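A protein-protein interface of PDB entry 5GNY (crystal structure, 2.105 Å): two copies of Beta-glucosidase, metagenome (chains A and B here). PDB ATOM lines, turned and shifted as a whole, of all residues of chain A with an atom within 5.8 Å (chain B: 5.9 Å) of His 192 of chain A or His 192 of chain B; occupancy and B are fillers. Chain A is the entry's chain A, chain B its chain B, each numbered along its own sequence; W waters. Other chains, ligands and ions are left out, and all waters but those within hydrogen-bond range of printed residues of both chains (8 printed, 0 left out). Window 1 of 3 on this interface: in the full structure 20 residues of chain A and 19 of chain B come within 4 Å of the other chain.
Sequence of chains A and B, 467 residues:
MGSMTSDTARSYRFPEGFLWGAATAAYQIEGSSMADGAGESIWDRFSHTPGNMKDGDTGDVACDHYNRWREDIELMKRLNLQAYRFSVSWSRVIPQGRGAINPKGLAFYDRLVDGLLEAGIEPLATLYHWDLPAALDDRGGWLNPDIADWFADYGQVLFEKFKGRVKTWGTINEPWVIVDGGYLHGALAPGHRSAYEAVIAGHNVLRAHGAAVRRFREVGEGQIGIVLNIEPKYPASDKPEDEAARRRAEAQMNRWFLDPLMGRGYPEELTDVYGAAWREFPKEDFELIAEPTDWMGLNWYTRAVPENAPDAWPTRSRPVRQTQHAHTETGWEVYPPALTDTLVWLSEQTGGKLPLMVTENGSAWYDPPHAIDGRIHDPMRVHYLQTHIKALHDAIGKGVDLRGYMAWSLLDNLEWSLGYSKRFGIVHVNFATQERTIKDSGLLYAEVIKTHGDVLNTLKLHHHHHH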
ATOM      1  N   ASP A 137     -21.734  -0.338  -5.555  1.00  0.00           N
ATOM      2  CA  ASP A 137     -22.873  -1.247  -5.578  1.00  0.00           C
ATOM      3  C   ASP A 137     -23.549  -1.228  -4.211  1.00  0.00           C
ATOM      4  O   ASP A 137     -24.773  -1.307  -4.107  1.00  0.00           O
ATOM      5  CB  ASP A 137     -22.434  -2.664  -5.943  1.00  0.00           C
ATOM      6  CG  ASP A 137     -23.587  -3.529  -6.419  1.00  0.00           C
ATOM      7  OD1 ASP A 137     -24.500  -2.998  -7.087  1.00  0.00           O
ATOM      8  OD2 ASP A 137     -23.574  -4.747  -6.139  1.00  0.00           O
ATOM      9  N   LEU A 143     -28.635   1.781  -9.687  1.00  0.00           N
ATOM     10  CA  LEU A 143     -29.956   2.198  -9.225  1.00  0.00           C
ATOM     11  C   LEU A 143     -29.906   3.569  -8.545  1.00  0.00           C
ATOM     12  O   LEU A 143     -30.929   4.239  -8.395  1.00  0.00           O
ATOM     13  CB  LEU A 143     -30.542   1.164  -8.262  1.00  0.00           C
ATOM     14  CG  LEU A 143     -30.664  -0.269  -8.784  1.00  0.00           C
ATOM     15  CD1 LEU A 143     -31.323  -1.152  -7.742  1.00  0.00           C
ATOM     16  CD2 LEU A 143     -31.434  -0.294 -10.095  1.00  0.00           C
ATOM     17  N   GLY A 181     -28.617  -8.441 -18.430  1.00  0.00           N
ATOM     18  CA  GLY A 181     -27.934  -9.501 -17.712  1.00  0.00           C
ATOM     19  C   GLY A 181     -27.816  -9.255 -16.217  1.00  0.00           C
ATOM     20  O   GLY A 181     -28.008 -10.166 -15.415  1.00  0.00           O
ATOM     21  N   GLY A 182     -27.509  -8.018 -15.838  1.00  0.00           N
ATOM     22  CA  GLY A 182     -27.191  -7.708 -14.456  1.00  0.00           C
ATOM     23  C   GLY A 182     -28.363  -7.355 -13.559  1.00  0.00           C
ATOM     24  O   GLY A 182     -28.302  -7.568 -12.348  1.00  0.00           O
ATOM     25  N   TYR A 183     -29.433  -6.818 -14.139  1.00  0.00           N
ATOM     26  CA  TYR A 183     -30.549  -6.341 -13.329  1.00  0.00           C
ATOM     27  C   TYR A 183     -31.887  -6.978 -13.690  1.00  0.00           C
ATOM     28  O   TYR A 183     -32.744  -7.141 -12.824  1.00  0.00           O
ATOM     29  CB  TYR A 183     -30.651  -4.813 -13.431  1.00  0.00           C
ATOM     30  CG  TYR A 183     -29.550  -4.102 -12.676  1.00  0.00           C
ATOM     31  CD1 TYR A 183     -28.332  -3.826 -13.283  1.00  0.00           C
ATOM     32  CD2 TYR A 183     -29.722  -3.725 -11.350  1.00  0.00           C
ATOM     33  CE1 TYR A 183     -27.315  -3.186 -12.591  1.00  0.00           C
ATOM     34  CE2 TYR A 183     -28.713  -3.085 -10.650  1.00  0.00           C
ATOM     35  CZ  TYR A 183     -27.511  -2.817 -11.277  1.00  0.00           C
ATOM     36  OH  TYR A 183     -26.505  -2.178 -10.586  1.00  0.00           O
ATOM     37  N   LEU A 184     -32.069  -7.338 -14.957  1.00  0.00           N
ATOM     38  CA  LEU A 184     -33.334  -7.917 -15.399  1.00  0.00           C
ATOM     39  C   LEU A 184     -33.401  -9.429 -15.157  1.00  0.00           C
ATOM     40  O   LEU A 184     -34.369  -9.922 -14.581  1.00  0.00           O
ATOM     41  CB  LEU A 184     -33.573  -7.619 -16.881  1.00  0.00           C
ATOM     42  CG  LEU A 184     -34.911  -8.112 -17.441  1.00  0.00           C
ATOM     43  CD1 LEU A 184     -36.075  -7.498 -16.667  1.00  0.00           C
ATOM     44  CD2 LEU A 184     -35.031  -7.811 -18.930  1.00  0.00           C
ATOM     45  N   HIS A 185     -32.373 -10.157 -15.588  1.00  0.00           N
ATOM     46  CA  HIS A 185     -32.389 -11.619 -15.497  1.00  0.00           C
ATOM     47  C   HIS A 185     -31.395 -12.208 -14.491  1.00  0.00           C
ATOM     48  O   HIS A 185     -31.549 -13.349 -14.069  1.00  0.00           O
ATOM     49  CB  HIS A 185     -32.139 -12.228 -16.878  1.00  0.00           C
ATOM     50  CG  HIS A 185     -33.225 -11.940 -17.865  1.00  0.00           C
ATOM     51  ND1 HIS A 185     -34.506 -12.431 -17.727  1.00  0.00           N
ATOM     52  CD2 HIS A 185     -33.224 -11.206 -19.003  1.00  0.00           C
ATOM     53  CE1 HIS A 185     -35.246 -12.015 -18.739  1.00  0.00           C
ATOM     54  NE2 HIS A 185     -34.492 -11.270 -19.528  1.00  0.00           N
ATOM     55  N   GLY A 186     -30.374 -11.444 -14.117  1.00  0.00           N
ATOM     56  CA  GLY A 186     -29.460 -11.867 -13.067  1.00  0.00           C
ATOM     57  C   GLY A 186     -28.392 -12.880 -13.441  1.00  0.00           C
ATOM     58  O   GLY A 186     -27.794 -13.504 -12.566  1.00  0.00           O
ATOM     59  N   ALA A 187     -28.140 -13.045 -14.733  1.00  0.00           N
ATOM     60  CA  ALA A 187     -27.117 -13.986 -15.179  1.00  0.00           C
ATOM     61  C   ALA A 187     -25.719 -13.392 -15.049  1.00  0.00           C
ATOM     62  O   ALA A 187     -24.723 -14.114 -15.082  1.00  0.00           O
ATOM     63  CB  ALA A 187     -27.375 -14.407 -16.612  1.00  0.00           C
ATOM     64  N   LEU A 188     -25.650 -12.072 -14.909  1.00  0.00           N
ATOM     65  CA  LEU A 188     -24.375 -11.379 -14.770  1.00  0.00           C
ATOM     66  C   LEU A 188     -24.381 -10.523 -13.513  1.00  0.00           C
ATOM     67  O   LEU A 188     -25.439 -10.251 -12.950  1.00  0.00           O
ATOM     68  CB  LEU A 188     -24.098 -10.507 -15.996  1.00  0.00           C
ATOM     69  CG  LEU A 188     -24.178 -11.183 -17.365  1.00  0.00           C
ATOM     70  CD1 LEU A 188     -24.086 -10.132 -18.454  1.00  0.00           C
ATOM     71  CD2 LEU A 188     -23.074 -12.211 -17.526  1.00  0.00           C
ATOM     72  N   ALA A 189     -23.199 -10.102 -13.072  1.00  0.00           N
ATOM     73  CA  ALA A 189     -23.091  -9.210 -11.921  1.00  0.00           C
ATOM     74  C   ALA A 189     -23.885  -7.928 -12.170  1.00  0.00           C
ATOM     75  O   ALA A 189     -23.902  -7.416 -13.288  1.00  0.00           O
ATOM     76  CB  ALA A 189     -21.632  -8.891 -11.633  1.00  0.00           C
ATOM     77  N   PRO A 190     -24.544  -7.397 -11.127  1.00  0.00           N
ATOM     78  CA  PRO A 190     -24.544  -7.848  -9.730  1.00  0.00           C
ATOM     79  C   PRO A 190     -25.557  -8.953  -9.418  1.00  0.00           C
ATOM     80  O   PRO A 190     -25.803  -9.234  -8.246  1.00  0.00           O
ATOM     81  CB  PRO A 190     -24.903  -6.574  -8.968  1.00  0.00           C
ATOM     82  CG  PRO A 190     -25.822  -5.858  -9.904  1.00  0.00           C
ATOM     83  CD  PRO A 190     -25.319  -6.154 -11.298  1.00  0.00           C
ATOM     84  N   GLY A 191     -26.141  -9.559 -10.447  1.00  0.00           N
ATOM     85  CA  GLY A 191     -27.032 -10.691 -10.259  1.00  0.00           C
ATOM     86  C   GLY A 191     -28.376 -10.358  -9.637  1.00  0.00           C
ATOM     87  O   GLY A 191     -28.850 -11.076  -8.760  1.00  0.00           O
ATOM     88  N   HIS A 192     -28.990  -9.268 -10.086  1.00  0.00           N
ATOM     89  CA  HIS A 192     -30.348  -8.933  -9.668  1.00  0.00           C
ATOM     90  C   HIS A 192     -31.348  -9.427 -10.707  1.00  0.00           C
ATOM     91  O   HIS A 192     -31.025  -9.526 -11.887  1.00  0.00           O
ATOM     92  CB  HIS A 192     -30.518  -7.421  -9.473  1.00  0.00           C
ATOM     93  CG  HIS A 192     -29.645  -6.839  -8.405  1.00  0.00           C
ATOM     94  ND1 HIS A 192     -29.831  -5.563  -7.909  1.00  0.00           N
ATOM     95  CD2 HIS A 192     -28.581  -7.345  -7.738  1.00  0.00           C
ATOM     96  CE1 HIS A 192     -28.922  -5.313  -6.987  1.00  0.00           C
ATOM     97  NE2 HIS A 192     -28.149  -6.380  -6.863  1.00  0.00           N
ATOM     98  N   ARG A 193     -32.565  -9.723 -10.272  1.00  0.00           N
ATOM     99  CA  ARG A 193     -33.613 -10.110 -11.205  1.00  0.00           C
ATOM    100  C   ARG A 193     -34.889  -9.332 -10.908  1.00  0.00           C
ATOM    101  O   ARG A 193     -35.664  -9.693 -10.021  1.00  0.00           O
ATOM    102  CB  ARG A 193     -33.867 -11.621 -11.144  1.00  0.00           C
ATOM    103  CG  ARG A 193     -34.930 -12.093 -12.120  1.00  0.00           C
ATOM    104  CD  ARG A 193     -34.972 -13.611 -12.242  1.00  0.00           C
ATOM    105  NE  ARG A 193     -36.081 -14.032 -13.092  1.00  0.00           N
ATOM    106  CZ  ARG A 193     -37.328 -14.197 -12.658  1.00  0.00           C
ATOM    107  NH1 ARG A 193     -37.617 -13.994 -11.380  1.00  0.00           N
ATOM    108  NH2 ARG A 193     -38.284 -14.572 -13.498  1.00  0.00           N
ATOM    109  N   SER A 194     -35.096  -8.255 -11.660  1.00  0.00           N
ATOM    110  CA  SER A 194     -36.202  -7.342 -11.411  1.00  0.00           C
ATOM    111  C   SER A 194     -36.416  -6.392 -12.581  1.00  0.00           C
ATOM    112  O   SER A 194     -35.480  -5.723 -13.024  1.00  0.00           O
ATOM    113  CB  SER A 194     -35.948  -6.535 -10.136  1.00  0.00           C
ATOM    114  OG  SER A 194     -36.860  -5.457 -10.026  1.00  0.00           O
ATOM    115  N   GLU A 197     -35.983  -2.732 -11.291  1.00  0.00           N
ATOM    116  CA  GLU A 197     -34.590  -2.314 -11.224  1.00  0.00           C
ATOM    117  C   GLU A 197     -33.981  -2.151 -12.611  1.00  0.00           C
ATOM    118  O   GLU A 197     -33.159  -1.261 -12.831  1.00  0.00           O
ATOM    119  CB  GLU A 197     -33.769  -3.309 -10.405  1.00  0.00           C
ATOM    120  CG  GLU A 197     -34.164  -3.364  -8.942  1.00  0.00           C
ATOM    121  CD  GLU A 197     -33.218  -4.209  -8.116  1.00  0.00           C
ATOM    122  OE1 GLU A 197     -32.200  -4.677  -8.667  1.00  0.00           O
ATOM    123  OE2 GLU A 197     -33.494  -4.406  -6.912  1.00  0.00           O
ATOM    124  N   ASP B 137     -33.709   1.273  -1.093  1.00  0.00           N
ATOM    125  CA  ASP B 137     -33.058   0.118  -1.701  1.00  0.00           C
ATOM    126  C   ASP B 137     -32.237   0.559  -2.906  1.00  0.00           C
ATOM    127  O   ASP B 137     -31.162   0.020  -3.169  1.00  0.00           O
ATOM    128  CB  ASP B 137     -34.084  -0.931  -2.123  1.00  0.00           C
ATOM    129  CG  ASP B 137     -33.460  -2.294  -2.368  1.00  0.00           C
ATOM    130  OD1 ASP B 137     -32.559  -2.689  -1.598  1.00  0.00           O
ATOM    131  OD2 ASP B 137     -33.871  -2.969  -3.334  1.00  0.00           O
ATOM    132  N   LEU B 143     -27.142  -2.218   2.588  1.00  0.00           N
ATOM    133  CA  LEU B 143     -25.723  -2.288   2.260  1.00  0.00           C
ATOM    134  C   LEU B 143     -25.071  -0.915   2.418  1.00  0.00           C
ATOM    135  O   LEU B 143     -23.847  -0.797   2.456  1.00  0.00           O
ATOM    136  CB  LEU B 143     -25.526  -2.819   0.839  1.00  0.00           C
ATOM    137  CG  LEU B 143     -26.157  -4.183   0.551  1.00  0.00           C
ATOM    138  CD1 LEU B 143     -25.922  -4.598  -0.894  1.00  0.00           C
ATOM    139  CD2 LEU B 143     -25.608  -5.232   1.508  1.00  0.00           C
ATOM    140  N   GLY B 181     -32.334 -14.470   4.191  1.00  0.00           N
ATOM    141  CA  GLY B 181     -33.292 -14.639   3.116  1.00  0.00           C
ATOM    142  C   GLY B 181     -33.175 -13.583   2.034  1.00  0.00           C
ATOM    143  O   GLY B 181     -33.301 -13.886   0.848  1.00  0.00           O
ATOM    144  N   GLY B 182     -32.927 -12.341   2.442  1.00  0.00           N
ATOM    145  CA  GLY B 182     -32.920 -11.223   1.518  1.00  0.00           C
ATOM    146  C   GLY B 182     -31.601 -10.937   0.823  1.00  0.00           C
ATOM    147  O   GLY B 182     -31.582 -10.338  -0.252  1.00  0.00           O
ATOM    148  N   TYR B 183     -30.495 -11.361   1.425  1.00  0.00           N
ATOM    149  CA  TYR B 183     -29.180 -11.010   0.896  1.00  0.00           C
ATOM    150  C   TYR B 183     -28.274 -12.210   0.665  1.00  0.00           C
ATOM    151  O   TYR B 183     -27.417 -12.187  -0.220  1.00  0.00           O
ATOM    152  CB  TYR B 183     -28.493 -10.015   1.834  1.00  0.00           C
ATOM    153  CG  TYR B 183     -29.085  -8.631   1.747  1.00  0.00           C
ATOM    154  CD1 TYR B 183     -30.117  -8.241   2.590  1.00  0.00           C
ATOM    155  CD2 TYR B 183     -28.627  -7.720   0.804  1.00  0.00           C
ATOM    156  CE1 TYR B 183     -30.667  -6.973   2.504  1.00  0.00           C
ATOM    157  CE2 TYR B 183     -29.172  -6.452   0.709  1.00  0.00           C
ATOM    158  CZ  TYR B 183     -30.190  -6.085   1.561  1.00  0.00           C
ATOM    159  OH  TYR B 183     -30.733  -4.823   1.465  1.00  0.00           O
ATOM    160  N   LEU B 184     -28.460 -13.260   1.456  1.00  0.00           N
ATOM    161  CA  LEU B 184     -27.584 -14.419   1.365  1.00  0.00           C
ATOM    162  C   LEU B 184     -28.082 -15.428   0.340  1.00  0.00           C
ATOM    163  O   LEU B 184     -27.307 -15.906  -0.489  1.00  0.00           O
ATOM    164  CB  LEU B 184     -27.439 -15.090   2.732  1.00  0.00           C
ATOM    165  CG  LEU B 184     -26.504 -16.300   2.791  1.00  0.00           C
ATOM    166  CD1 LEU B 184     -25.106 -15.925   2.310  1.00  0.00           C
ATOM    167  CD2 LEU B 184     -26.456 -16.870   4.204  1.00  0.00           C
ATOM    168  N   HIS B 185     -29.373 -15.745   0.396  1.00  0.00           N
ATOM    169  CA  HIS B 185     -29.935 -16.805  -0.442  1.00  0.00           C
ATOM    170  C   HIS B 185     -30.931 -16.284  -1.477  1.00  0.00           C
ATOM    171  O   HIS B 185     -31.214 -16.961  -2.460  1.00  0.00           O
ATOM    172  CB  HIS B 185     -30.600 -17.871   0.430  1.00  0.00           C
ATOM    173  CG  HIS B 185     -29.635 -18.649   1.272  1.00  0.00           C
ATOM    174  ND1 HIS B 185     -28.716 -19.522   0.731  1.00  0.00           N
ATOM    175  CD2 HIS B 185     -29.444 -18.683   2.612  1.00  0.00           C
ATOM    176  CE1 HIS B 185     -27.999 -20.061   1.701  1.00  0.00           C
ATOM    177  NE2 HIS B 185     -28.422 -19.570   2.853  1.00  0.00           N
ATOM    178  N   GLY B 186     -31.465 -15.087  -1.249  1.00  0.00           N
ATOM    179  CA  GLY B 186     -32.314 -14.437  -2.233  1.00  0.00           C
ATOM    180  C   GLY B 186     -33.749 -14.926  -2.308  1.00  0.00           C
ATOM    181  O   GLY B 186     -34.441 -14.677  -3.294  1.00  0.00           O
ATOM    182  N   ALA B 187     -34.206 -15.608  -1.264  1.00  0.00           N
ATOM    183  CA  ALA B 187     -35.570 -16.121  -1.229  1.00  0.00           C
ATOM    184  C   ALA B 187     -36.569 -15.024  -0.875  1.00  0.00           C
ATOM    185  O   ALA B 187     -37.762 -15.152  -1.141  1.00  0.00           O
ATOM    186  CB  ALA B 187     -35.677 -17.274  -0.239  1.00  0.00           C
ATOM    187  N   LEU B 188     -36.073 -13.950  -0.270  1.00  0.00           N
ATOM    188  CA  LEU B 188     -36.918 -12.834   0.139  1.00  0.00           C
ATOM    189  C   LEU B 188     -36.418 -11.528  -0.457  1.00  0.00           C
ATOM    190  O   LEU B 188     -35.270 -11.439  -0.882  1.00  0.00           O
ATOM    191  CB  LEU B 188     -36.953 -12.720   1.661  1.00  0.00           C
ATOM    192  CG  LEU B 188     -37.333 -13.978   2.436  1.00  0.00           C
ATOM    193  CD1 LEU B 188     -37.123 -13.741   3.918  1.00  0.00           C
ATOM    194  CD2 LEU B 188     -38.774 -14.372   2.150  1.00  0.00           C
ATOM    195  N   ALA B 189     -37.282 -10.517  -0.479  1.00  0.00           N
ATOM    196  CA  ALA B 189     -36.890  -9.177  -0.911  1.00  0.00           C
ATOM    197  C   ALA B 189     -35.690  -8.697  -0.099  1.00  0.00           C
ATOM    198  O   ALA B 189     -35.632  -8.929   1.107  1.00  0.00           O
ATOM    199  CB  ALA B 189     -38.054  -8.211  -0.764  1.00  0.00           C
ATOM    200  N   PRO B 190     -34.732  -8.019  -0.752  1.00  0.00           N
ATOM    201  CA  PRO B 190     -34.759  -7.623  -2.164  1.00  0.00           C
ATOM    202  C   PRO B 190     -34.224  -8.692  -3.120  1.00  0.00           C
ATOM    203  O   PRO B 190     -34.001  -8.397  -4.293  1.00  0.00           O
ATOM    204  CB  PRO B 190     -33.864  -6.383  -2.184  1.00  0.00           C
ATOM    205  CG  PRO B 190     -32.854  -6.654  -1.121  1.00  0.00           C
ATOM    206  CD  PRO B 190     -33.551  -7.475  -0.055  1.00  0.00           C
ATOM    207  N   GLY B 191     -34.016  -9.907  -2.626  1.00  0.00           N
ATOM    208  CA  GLY B 191     -33.652 -11.019  -3.486  1.00  0.00           C
ATOM    209  C   GLY B 191     -32.227 -11.014  -4.003  1.00  0.00           C
ATOM    210  O   GLY B 191     -31.989 -11.323  -5.170  1.00  0.00           O
ATOM    211  N   HIS B 192     -31.278 -10.663  -3.140  1.00  0.00           N
ATOM    212  CA  HIS B 192     -29.863 -10.751  -3.488  1.00  0.00           C
ATOM    213  C   HIS B 192     -29.297 -12.082  -3.007  1.00  0.00           C
ATOM    214  O   HIS B 192     -29.760 -12.636  -2.013  1.00  0.00           O
ATOM    215  CB  HIS B 192     -29.057  -9.602  -2.873  1.00  0.00           C
ATOM    216  CG  HIS B 192     -29.480  -8.239  -3.331  1.00  0.00           C
ATOM    217  ND1 HIS B 192     -28.678  -7.128  -3.183  1.00  0.00           N
ATOM    218  CD2 HIS B 192     -30.620  -7.803  -3.917  1.00  0.00           C
ATOM    219  CE1 HIS B 192     -29.303  -6.067  -3.663  1.00  0.00           C
ATOM    220  NE2 HIS B 192     -30.486  -6.450  -4.113  1.00  0.00           N
ATOM    221  N   ARG B 193     -28.289 -12.588  -3.706  1.00  0.00           N
ATOM    222  CA  ARG B 193     -27.639 -13.830  -3.299  1.00  0.00           C
ATOM    223  C   ARG B 193     -26.130 -13.645  -3.231  1.00  0.00           C
ATOM    224  O   ARG B 193     -25.428 -13.817  -4.227  1.00  0.00           O
ATOM    225  CB  ARG B 193     -27.994 -14.964  -4.258  1.00  0.00           C
ATOM    226  CG  ARG B 193     -27.402 -16.312  -3.876  1.00  0.00           C
ATOM    227  CD  ARG B 193     -28.000 -17.436  -4.712  1.00  0.00           C
ATOM    228  NE  ARG B 193     -27.378 -18.720  -4.407  1.00  0.00           N
ATOM    229  CZ  ARG B 193     -26.251 -19.153  -4.966  1.00  0.00           C
ATOM    230  NH1 ARG B 193     -25.625 -18.406  -5.865  1.00  0.00           N
ATOM    231  NH2 ARG B 193     -25.751 -20.334  -4.628  1.00  0.00           N
ATOM    232  N   SER B 194     -25.638 -13.296  -2.046  1.00  0.00           N
ATOM    233  CA  SER B 194     -24.225 -12.986  -1.865  1.00  0.00           C
ATOM    234  C   SER B 194     -23.817 -13.052  -0.396  1.00  0.00           C
ATOM    235  O   SER B 194     -24.454 -12.438   0.461  1.00  0.00           O
ATOM    236  CB  SER B 194     -23.917 -11.597  -2.430  1.00  0.00           C
ATOM    237  OG  SER B 194     -22.614 -11.169  -2.070  1.00  0.00           O
ATOM    238  N   GLU B 197     -22.504  -9.498   0.600  1.00  0.00           N
ATOM    239  CA  GLU B 197     -23.545  -8.541   0.944  1.00  0.00           C
ATOM    240  C   GLU B 197     -24.212  -8.897   2.269  1.00  0.00           C
ATOM    241  O   GLU B 197     -24.620  -8.013   3.023  1.00  0.00           O
ATOM    242  CB  GLU B 197     -24.587  -8.461  -0.174  1.00  0.00           C
ATOM    243  CG  GLU B 197     -24.013  -8.021  -1.515  1.00  0.00           C
ATOM    244  CD  GLU B 197     -25.087  -7.714  -2.543  1.00  0.00           C
ATOM    245  OE1 GLU B 197     -26.280  -7.705  -2.179  1.00  0.00           O
ATOM    246  OE2 GLU B 197     -24.737  -7.483  -3.718  1.00  0.00           O
HETATM  247  O   HOH W   1     -25.488  -9.576  -5.563  1.00  0.00           O
HETATM  248  O   HOH W   2     -27.406 -11.250  -6.285  1.00  0.00           O
HETATM  249  O   HOH W   3     -22.538  -6.940  -5.187  1.00  0.00           O
HETATM  250  O   HOH W   4     -26.150  -5.662  -5.277  1.00  0.00           O
HETATM  251  O   HOH W   5     -31.962  -4.342  -4.835  1.00  0.00           O
HETATM  252  O   HOH W   6     -33.690  -7.151  -6.417  1.00  0.00           O
HETATM  253  O   HOH W   7     -32.951  -9.668  -7.540  1.00  0.00           O
HETATM  254  O   HOH W   8     -35.553  -3.607  -5.187  1.00  0.00           O
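Water W6 bridges O of Pro 190 of chain B (2.5 Å) and OE2 of Glu 197 of chain A (2.8 Å). Water W8 bridges OD2 of Asp 137 of chain B (2.6 Å) and OE2 of Glu 197 of chain A (2.8 Å). Water W3 bridges OD2 of Asp 137 of chain A (2.6 Å) and OE2 of Glu 197 of chain B (2.7 Å). Water W1 bridges O of Pro 190 of chain A and OE2 of Glu 197 of chain B. Water W7 bridges the backbone NH (N) of Arg 193 of chain A and the backbone carbonyl oxygen (O) of Gly 191 of chain B. Water W2 lies within hydrogen-bond range of O of Gly 191 of chain A (2.9 Å), N of Arg 193 of chain B (3.0 Å) and O of Pro 190 of chain A (3.2 Å).
Asp 137 of chain A touches Glu 197 of chain B, and with the chains exchanged Glu 197 of chain A touches Asp 137 of chain B. His 192 of chain B touches its own counterpart, His 192 of chain A. Positions printed for both chains: 137, 143, 181, 182, 183, 184, 185, 186, 187, 188, 189, 190, 191, 192, 193, 194 and 197.
A ring nitrogen (ND1) of His 192 of chain A lies within hydrogen-bond range of the side-chain carboxylate (OE1) of Glu 197 of chain A (2.6 Å). N of His 192 of chain B is in hydrogen-bond range of O of Gly 182 of chain B, at 2.9 Å. The backbone carbonyl oxygen (O) of His 192 of chain A sits at hydrogen-bond distance from the backbone NH (N) of Gly 186 of chain A (3.0 Å). OG of Ser 194 of chain B lies within hydrogen-bond range of N of Glu 197 of chain B (3.2 Å). O of Gly 182 of chain A sits at hydrogen-bond distance from N of His 192 of chain A (2.9 Å). The side-chain hydroxyl (OG) of Ser 194 of chain A lies within hydrogen-bond range of the backbone NH (N) of Glu 197 of chain A (3.1 Å).
Hydrophobic or aromatic side chains of chain B that line the printed part of chain A: His 192. Along chain B the printed residues that touch a printed residue of chain A span positions 137 to 197. Of the 17 printed residues of chain A, 3 touch a printed residue of chain B. Printed residues of chain A that touch a printed residue of chain B: Asp 137, His 192 and Glu 197. Hydrophobic or aromatic side chains of chain A within 4 Å of the printed part of chain B: His 192. Among the printed residues, no Asp or Glu carboxylate lies within 4 Å of a Lys or Arg side-chain nitrogen of the other chain.
Among the printed residues, pairs that only touch across the chains: His 192 of chain A with His 192 of chain B (3.4 Å), Asp 137 of chain A with Glu 197 of chain B (3.8 Å) and Glu 197 of chain A with Asp 137 of chain B (3.9 Å).
Of the printed residues of chain B, Asp 137 of chain A touches Glu 197 (3.8 Å). Gly 181 of chain A touches none of the printed residues of chain B. Pro 190 of chain A touches none of the printed residues of chain B. Of chain B, only His 192 comes within 4 Å of His 192 of chain A. Of the printed residues of chain B, Glu 197 of chain A touches Asp 137. Printed residues of chain A within 4 Å of Asp 137 of chain B: Glu 197 (3.9 Å). Printed residues of chain A within 4 Å of Glu 197 of chain B: Asp 137 (3.8 Å). The nearest residue of chain A that does not touch His 192 of chain B is Glu 197 of chain A (4.6 Å). The nearest printed residue of chain B that does not touch Glu 197 of chain A is His 192 of chain B (4.6 Å).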
